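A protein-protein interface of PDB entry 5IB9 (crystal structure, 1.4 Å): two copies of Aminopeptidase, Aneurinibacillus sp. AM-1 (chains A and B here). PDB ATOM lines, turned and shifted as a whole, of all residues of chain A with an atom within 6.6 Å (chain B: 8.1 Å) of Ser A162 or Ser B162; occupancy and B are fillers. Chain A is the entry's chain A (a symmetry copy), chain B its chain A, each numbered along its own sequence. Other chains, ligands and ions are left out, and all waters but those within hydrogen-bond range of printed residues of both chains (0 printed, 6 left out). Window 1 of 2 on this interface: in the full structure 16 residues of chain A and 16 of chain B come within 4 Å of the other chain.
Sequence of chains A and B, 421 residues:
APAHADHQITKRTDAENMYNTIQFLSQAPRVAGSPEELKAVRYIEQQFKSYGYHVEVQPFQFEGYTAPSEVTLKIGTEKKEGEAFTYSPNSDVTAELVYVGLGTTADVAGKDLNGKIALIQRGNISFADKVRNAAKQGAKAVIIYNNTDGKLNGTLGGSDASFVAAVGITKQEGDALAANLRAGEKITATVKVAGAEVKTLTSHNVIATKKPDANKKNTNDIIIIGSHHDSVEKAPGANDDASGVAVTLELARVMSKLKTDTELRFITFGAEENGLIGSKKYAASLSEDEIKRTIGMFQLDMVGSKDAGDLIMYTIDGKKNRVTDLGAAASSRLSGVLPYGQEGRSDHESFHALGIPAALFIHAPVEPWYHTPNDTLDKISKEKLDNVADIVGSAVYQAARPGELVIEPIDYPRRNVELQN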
ATOM      1  N   PRO A  89       8.543 -16.408  26.344  1.00  0.00           N
ATOM      2  CA  PRO A  89       9.598 -15.492  26.665  1.00  0.00           C
ATOM      3  C   PRO A  89      10.148 -15.795  28.096  1.00  0.00           C
ATOM      4  O   PRO A  89       9.490 -16.515  28.865  1.00  0.00           O
ATOM      5  CB  PRO A  89       8.903 -14.148  26.567  1.00  0.00           C
ATOM      6  CG  PRO A  89       7.667 -14.384  25.722  1.00  0.00           C
ATOM      7  CD  PRO A  89       7.268 -15.724  26.065  1.00  0.00           C
ATOM      8  N   VAL A 131      -2.298 -15.154  25.741  1.00  0.00           N
ATOM      9  CA  VAL A 131      -1.076 -14.427  26.122  1.00  0.00           C
ATOM     10  C   VAL A 131      -1.028 -13.019  25.485  1.00  0.00           C
ATOM     11  O   VAL A 131      -0.679 -12.000  26.139  1.00  0.00           O
ATOM     12  CB  VAL A 131       0.193 -15.272  25.834  1.00  0.00           C
ATOM     13  CG1 VAL A 131       1.449 -14.478  26.127  1.00  0.00           C
ATOM     14  CG2 VAL A 131       0.163 -16.536  26.670  1.00  0.00           C
ATOM     15  N   ARG A 132      -1.293 -12.931  24.177  1.00  0.00           N
ATOM     16  CA  ARG A 132      -1.235 -11.613  23.535  1.00  0.00           C
ATOM     17  C   ARG A 132      -2.308 -10.637  24.073  1.00  0.00           C
ATOM     18  O   ARG A 132      -2.022  -9.460  24.315  1.00  0.00           O
ATOM     19  CB  ARG A 132      -1.377 -11.759  22.005  1.00  0.00           C
ATOM     20  CG  ARG A 132      -0.087 -12.115  21.262  1.00  0.00           C
ATOM     21  CD  ARG A 132      -0.353 -12.087  19.743  1.00  0.00           C
ATOM     22  NE  ARG A 132      -1.230 -13.193  19.395  1.00  0.00           N
ATOM     23  CZ  ARG A 132      -0.828 -14.307  18.779  1.00  0.00           C
ATOM     24  NH1 ARG A 132       0.453 -14.464  18.384  1.00  0.00           N
ATOM     25  NH2 ARG A 132      -1.721 -15.276  18.540  1.00  0.00           N
ATOM     26  N   ALA A 135      -0.958  -9.437  27.428  1.00  0.00           N
ATOM     27  CA  ALA A 135       0.228  -8.627  27.212  1.00  0.00           C
ATOM     28  C   ALA A 135      -0.121  -7.244  26.603  1.00  0.00           C
ATOM     29  O   ALA A 135       0.528  -6.263  26.896  1.00  0.00           O
ATOM     30  CB  ALA A 135       1.242  -9.356  26.334  1.00  0.00           C
ATOM     31  N   LYS A 136      -1.168  -7.186  25.793  1.00  0.00           N
ATOM     32  CA  LYS A 136      -1.595  -5.914  25.158  1.00  0.00           C
ATOM     33  C   LYS A 136      -2.083  -4.962  26.258  1.00  0.00           C
ATOM     34  O   LYS A 136      -2.032  -3.735  26.089  1.00  0.00           O
ATOM     35  CB  LYS A 136      -2.707  -6.186  24.103  1.00  0.00           C
ATOM     36  CG  LYS A 136      -3.097  -4.993  23.187  1.00  0.00           C
ATOM     37  CD  LYS A 136      -2.279  -4.969  21.886  1.00  0.00           C
ATOM     38  CE  LYS A 136      -2.315  -3.599  21.180  1.00  0.00           C
ATOM     39  NZ  LYS A 136      -0.995  -3.329  20.480  1.00  0.00           N
ATOM     40  N   ASP A 160       7.226 -15.229  18.953  1.00  0.00           N
ATOM     41  CA  ASP A 160       6.447 -13.992  18.877  1.00  0.00           C
ATOM     42  C   ASP A 160       6.752 -13.034  20.019  1.00  0.00           C
ATOM     43  O   ASP A 160       6.536 -13.361  21.193  1.00  0.00           O
ATOM     44  CB  ASP A 160       4.931 -14.261  18.792  1.00  0.00           C
ATOM     45  CG  ASP A 160       4.117 -12.986  18.536  1.00  0.00           C
ATOM     46  OD1 ASP A 160       4.711 -11.886  18.619  1.00  0.00           O
ATOM     47  OD2 ASP A 160       2.892 -13.072  18.240  1.00  0.00           O
ATOM     48  N   ALA A 161       7.225 -11.835  19.673  1.00  0.00           N
ATOM     49  CA  ALA A 161       7.707 -10.890  20.678  1.00  0.00           C
ATOM     50  C   ALA A 161       6.571 -10.057  21.274  1.00  0.00           C
ATOM     51  O   ALA A 161       6.780  -9.210  22.156  1.00  0.00           O
ATOM     52  CB  ALA A 161       8.830  -9.998  20.111  1.00  0.00           C
ATOM     53  N   SER A 162       5.357 -10.328  20.814  1.00  0.00           N
ATOM     54  CA  SER A 162       4.186  -9.782  21.487  1.00  0.00           C
ATOM     55  C   SER A 162       3.939 -10.522  22.795  1.00  0.00           C
ATOM     56  O   SER A 162       3.307  -9.970  23.708  1.00  0.00           O
ATOM     57  CB  SER A 162       2.963  -9.907  20.628  1.00  0.00           C
ATOM     58  OG  SER A 162       3.384  -9.632  19.319  1.00  0.00           O
ATOM     59  N   PHE A 163       4.426 -11.752  22.870  1.00  0.00           N
ATOM     60  CA  PHE A 163       4.227 -12.560  24.097  1.00  0.00           C
ATOM     61  C   PHE A 163       4.923 -12.036  25.367  1.00  0.00           C
ATOM     62  O   PHE A 163       5.855 -11.202  25.355  1.00  0.00           O
ATOM     63  CB  PHE A 163       4.666 -13.997  23.881  1.00  0.00           C
ATOM     64  CG  PHE A 163       3.941 -14.758  22.784  1.00  0.00           C
ATOM     65  CD1 PHE A 163       2.590 -14.554  22.483  1.00  0.00           C
ATOM     66  CD2 PHE A 163       4.636 -15.764  22.113  1.00  0.00           C
ATOM     67  CE1 PHE A 163       1.961 -15.339  21.501  1.00  0.00           C
ATOM     68  CE2 PHE A 163       4.010 -16.544  21.141  1.00  0.00           C
ATOM     69  CZ  PHE A 163       2.673 -16.310  20.838  1.00  0.00           C
ATOM     70  N   VAL A 164       4.444 -12.542  26.506  1.00  0.00           N
ATOM     71  CA  VAL A 164       5.225 -12.388  27.751  1.00  0.00           C
ATOM     72  C   VAL A 164       5.252 -13.768  28.283  1.00  0.00           C
ATOM     73  O   VAL A 164       4.550 -14.622  27.773  1.00  0.00           O
ATOM     74  CB  VAL A 164       4.597 -11.418  28.801  1.00  0.00           C
ATOM     75  CG1 VAL A 164       4.600 -10.002  28.268  1.00  0.00           C
ATOM     76  CG2 VAL A 164       3.192 -11.884  29.205  1.00  0.00           C
ATOM     77  N   PRO B  89      -1.634   0.367  12.822  1.00  0.00           N
ATOM     78  CA  PRO B  89      -2.879   0.136  13.494  1.00  0.00           C
ATOM     79  C   PRO B  89      -3.711   1.458  13.540  1.00  0.00           C
ATOM     80  O   PRO B  89      -3.154   2.541  13.297  1.00  0.00           O
ATOM     81  CB  PRO B  89      -2.427  -0.330  14.865  1.00  0.00           C
ATOM     82  CG  PRO B  89      -0.996  -0.798  14.689  1.00  0.00           C
ATOM     83  CD  PRO B  89      -0.469   0.081  13.678  1.00  0.00           C
ATOM     84  N   ALA B 128       9.528  -0.392  11.883  1.00  0.00           N
ATOM     85  CA  ALA B 128       8.976  -1.494  12.680  1.00  0.00           C
ATOM     86  C   ALA B 128       9.517  -1.654  14.107  1.00  0.00           C
ATOM     87  O   ALA B 128       8.750  -1.818  15.053  1.00  0.00           O
ATOM     88  CB  ALA B 128       9.181  -2.839  11.901  1.00  0.00           C
ATOM     89  N   VAL B 131       8.616   1.243  16.512  1.00  0.00           N
ATOM     90  CA  VAL B 131       7.231   1.108  16.989  1.00  0.00           C
ATOM     91  C   VAL B 131       7.101  -0.003  18.057  1.00  0.00           C
ATOM     92  O   VAL B 131       6.425   0.155  19.108  1.00  0.00           O
ATOM     93  CB  VAL B 131       6.243   0.937  15.805  1.00  0.00           C
ATOM     94  CG1 VAL B 131       4.835   0.692  16.306  1.00  0.00           C
ATOM     95  CG2 VAL B 131       6.281   2.174  14.928  1.00  0.00           C
ATOM     96  N   ARG B 132       7.668  -1.183  17.782  1.00  0.00           N
ATOM     97  CA  ARG B 132       7.545  -2.267  18.764  1.00  0.00           C
ATOM     98  C   ARG B 132       8.259  -1.950  20.099  1.00  0.00           C
ATOM     99  O   ARG B 132       7.722  -2.215  21.178  1.00  0.00           O
ATOM    100  CB  ARG B 132       8.092  -3.584  18.174  1.00  0.00           C
ATOM    101  CG  ARG B 132       7.115  -4.354  17.284  1.00  0.00           C
ATOM    102  CD  ARG B 132       7.747  -5.704  16.887  1.00  0.00           C
ATOM    103  NE  ARG B 132       8.862  -5.459  15.988  1.00  0.00           N
ATOM    104  CZ  ARG B 132       8.830  -5.679  14.671  1.00  0.00           C
ATOM    105  NH1 ARG B 132       7.738  -6.204  14.077  1.00  0.00           N
ATOM    106  NH2 ARG B 132       9.909  -5.382  13.936  1.00  0.00           N
ATOM    107  N   ASN B 133       9.441  -1.352  20.024  1.00  0.00           N
ATOM    108  CA  ASN B 133      10.178  -0.979  21.258  1.00  0.00           C
ATOM    109  C   ASN B 133       9.351  -0.042  22.160  1.00  0.00           C
ATOM    110  O   ASN B 133       9.265  -0.259  23.377  1.00  0.00           O
ATOM    111  CB  ASN B 133      11.538  -0.358  20.936  1.00  0.00           C
ATOM    112  CG  ASN B 133      12.503  -1.338  20.233  1.00  0.00           C
ATOM    113  OD1 ASN B 133      13.404  -0.901  19.499  1.00  0.00           O
ATOM    114  ND2 ASN B 133      12.264  -2.646  20.393  1.00  0.00           N
ATOM    115  N   ALA B 134       8.707   0.957  21.546  1.00  0.00           N
ATOM    116  CA  ALA B 134       7.820   1.911  22.272  1.00  0.00           C
ATOM    117  C   ALA B 134       6.543   1.260  22.789  1.00  0.00           C
ATOM    118  O   ALA B 134       6.122   1.499  23.946  1.00  0.00           O
ATOM    119  CB  ALA B 134       7.508   3.138  21.361  1.00  0.00           C
ATOM    120  N   ALA B 135       5.918   0.431  21.933  1.00  0.00           N
ATOM    121  CA  ALA B 135       4.702  -0.273  22.302  1.00  0.00           C
ATOM    122  C   ALA B 135       4.948  -1.280  23.456  1.00  0.00           C
ATOM    123  O   ALA B 135       4.084  -1.489  24.281  1.00  0.00           O
ATOM    124  CB  ALA B 135       4.086  -0.981  21.098  1.00  0.00           C
ATOM    125  N   LYS B 136       6.138  -1.858  23.513  1.00  0.00           N
ATOM    126  CA  LYS B 136       6.483  -2.834  24.577  1.00  0.00           C
ATOM    127  C   LYS B 136       6.504  -2.098  25.923  1.00  0.00           C
ATOM    128  O   LYS B 136       6.284  -2.715  26.975  1.00  0.00           O
ATOM    129  CB  LYS B 136       7.856  -3.502  24.270  1.00  0.00           C
ATOM    130  CG  LYS B 136       8.250  -4.711  25.162  1.00  0.00           C
ATOM    131  CD  LYS B 136       7.797  -6.050  24.558  1.00  0.00           C
ATOM    132  CE  LYS B 136       7.770  -7.195  25.590  1.00  0.00           C
ATOM    133  NZ  LYS B 136       6.644  -8.164  25.278  1.00  0.00           N
ATOM    134  N   ALA B 139       3.519   2.652  25.134  1.00  0.00           N
ATOM    135  CA  ALA B 139       3.134   3.728  24.210  1.00  0.00           C
ATOM    136  C   ALA B 139       1.837   3.370  23.512  1.00  0.00           C
ATOM    137  O   ALA B 139       1.656   2.241  23.080  1.00  0.00           O
ATOM    138  CB  ALA B 139       4.228   4.016  23.207  1.00  0.00           C
ATOM    139  N   LEU B 156       5.958  -0.342   8.091  1.00  0.00           N
ATOM    140  CA  LEU B 156       6.331  -1.165   9.203  1.00  0.00           C
ATOM    141  C   LEU B 156       6.599  -2.566   8.673  1.00  0.00           C
ATOM    142  O   LEU B 156       6.898  -3.499   9.433  1.00  0.00           O
ATOM    143  CB  LEU B 156       5.234  -1.130  10.264  1.00  0.00           C
ATOM    144  CG  LEU B 156       4.848   0.312  10.669  1.00  0.00           C
ATOM    145  CD1 LEU B 156       3.881   0.134  11.793  1.00  0.00           C
ATOM    146  CD2 LEU B 156       6.071   1.119  11.104  1.00  0.00           C
ATOM    147  N   SER B 159       2.092  -6.769   8.433  1.00  0.00           N
ATOM    148  CA  SER B 159       1.065  -6.787   9.454  1.00  0.00           C
ATOM    149  C   SER B 159       1.705  -7.182  10.752  1.00  0.00           C
ATOM    150  O   SER B 159       2.618  -8.026  10.772  1.00  0.00           O
ATOM    151  CB  SER B 159      -0.034  -7.800   9.071  1.00  0.00           C
ATOM    152  OG  SER B 159       0.505  -9.014   8.503  1.00  0.00           O
ATOM    153  N   ASP B 160       1.282  -6.584  11.850  1.00  0.00           N
ATOM    154  CA  ASP B 160       1.827  -6.975  13.152  1.00  0.00           C
ATOM    155  C   ASP B 160       1.081  -6.342  14.316  1.00  0.00           C
ATOM    156  O   ASP B 160       1.047  -5.112  14.451  1.00  0.00           O
ATOM    157  CB  ASP B 160       3.338  -6.689  13.261  1.00  0.00           C
ATOM    158  CG  ASP B 160       3.954  -7.253  14.548  1.00  0.00           C
ATOM    159  OD1 ASP B 160       3.176  -7.688  15.429  1.00  0.00           O
ATOM    160  OD2 ASP B 160       5.210  -7.277  14.684  1.00  0.00           O
ATOM    161  N   ALA B 161       0.509  -7.184  15.179  1.00  0.00           N
ATOM    162  CA  ALA B 161      -0.369  -6.701  16.243  1.00  0.00           C
ATOM    163  C   ALA B 161       0.416  -6.267  17.482  1.00  0.00           C
ATOM    164  O   ALA B 161      -0.153  -5.813  18.486  1.00  0.00           O
ATOM    165  CB  ALA B 161      -1.450  -7.744  16.591  1.00  0.00           C
ATOM    166  N   SER B 162       1.735  -6.374  17.393  1.00  0.00           N
ATOM    167  CA  SER B 162       2.585  -5.759  18.404  1.00  0.00           C
ATOM    168  C   SER B 162       2.618  -4.249  18.213  1.00  0.00           C
ATOM    169  O   SER B 162       2.892  -3.510  19.170  1.00  0.00           O
ATOM    170  CB  SER B 162       3.987  -6.283  18.323  1.00  0.00           C
ATOM    171  OG  SER B 162       3.869  -7.653  18.045  1.00  0.00           O
ATOM    172  N   PHE B 163       2.350  -3.810  16.992  1.00  0.00           N
ATOM    173  CA  PHE B 163       2.370  -2.356  16.700  1.00  0.00           C
ATOM    174  C   PHE B 163       1.295  -1.513  17.412  1.00  0.00           C
ATOM    175  O   PHE B 163       0.266  -1.995  17.932  1.00  0.00           O
ATOM    176  CB  PHE B 163       2.257  -2.097  15.208  1.00  0.00           C
ATOM    177  CG  PHE B 163       3.358  -2.690  14.344  1.00  0.00           C
ATOM    178  CD1 PHE B 163       4.683  -2.804  14.775  1.00  0.00           C
ATOM    179  CD2 PHE B 163       3.042  -3.051  13.035  1.00  0.00           C
ATOM    180  CE1 PHE B 163       5.667  -3.299  13.901  1.00  0.00           C
ATOM    181  CE2 PHE B 163       4.018  -3.539  12.168  1.00  0.00           C
ATOM    182  CZ  PHE B 163       5.327  -3.669  12.622  1.00  0.00           C
ATOM    183  N   VAL B 164       1.551  -0.203  17.437  1.00  0.00           N
ATOM    184  CA  VAL B 164       0.467   0.740  17.781  1.00  0.00           C
ATOM    185  C   VAL B 164       0.547   1.732  16.687  1.00  0.00           C
ATOM    186  O   VAL B 164       1.493   1.705  15.921  1.00  0.00           O
ATOM    187  CB  VAL B 164       0.629   1.448  19.163  1.00  0.00           C
ATOM    188  CG1 VAL B 164       0.514   0.437  20.283  1.00  0.00           C
ATOM    189  CG2 VAL B 164       1.946   2.234  19.223  1.00  0.00           C
ATOM    190  N   ALA B 165      -0.437   2.641  16.590  1.00  0.00           N
ATOM    191  CA  ALA B 165      -0.464   3.561  15.471  1.00  0.00           C
ATOM    192  C   ALA B 165       0.864   4.312  15.338  1.00  0.00           C
ATOM    193  O   ALA B 165       1.471   4.700  16.351  1.00  0.00           O
ATOM    194  CB  ALA B 165      -1.672   4.544  15.616  1.00  0.00           C
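The side-chain amino group of Lys B136 sits at hydrogen-bond distance from the backbone carbonyl oxygen of Ala A161 (3.3 Å). The side-chain hydroxyl (OG) of Ser B162 lies within hydrogen-bond range of the side-chain hydroxyl (OG) of Ser A162 (2.4 Å). The backbone carbonyl oxygen of Phe B163 lies within hydrogen-bond range of the side-chain amino group of Lys A136, 3.1 Å away. NZ of Lys A136 lies within hydrogen-bond range of O of Ala B161 (3.3 Å). The side-chain amino group of Lys B136 is in hydrogen-bond range of the backbone carbonyl oxygen of Phe A163 (3.1 Å).
OD1 of Asp A160 lies within hydrogen-bond range of OG of Ser A162, 2.7 Å away. The side-chain carboxylate of Asp B160 is in hydrogen-bond range of the side-chain hydroxyl of Ser B162 (2.7 Å).
Of chain B, only Ser B162 (2.4 Å) comes within 4 Å of Ser A162. Of the printed residues of chain A, Lys B136 touches Ala A161 (3.3 Å) and Phe A163 (3.1 Å). Ala B139 touches none of the printed residues of chain A. Of chain A, only Ser A162 (2.4 Å) comes within 4 Å of Ser B162. Of the printed residues of chain A, Phe B163 touches Lys A136. The nearest residue of chain B that does not touch Ser A162 is Lys B136 (4.1 Å).
Among the printed residues, 5 pairs touch across the chains. Among the printed residues, no Asp or Glu carboxylate lies within 4 Å of a Lys or Arg side-chain nitrogen of the other chain.
Lys A136 touches Ala B161, and with the chains exchanged Ala A161 touches Lys B136. Lys A136 touches Phe B163, and with the chains exchanged Phe A163 touches Lys B136. Ser A162 touches its own counterpart, Ser B162. Positions printed for both chains: 89, 131, 132, 135, 136, 160, 161, 162, 163 and 164. Of the 5 pairs that touch across the chains among the printed residues, 5 have their exchanged pair printed and touching as well.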
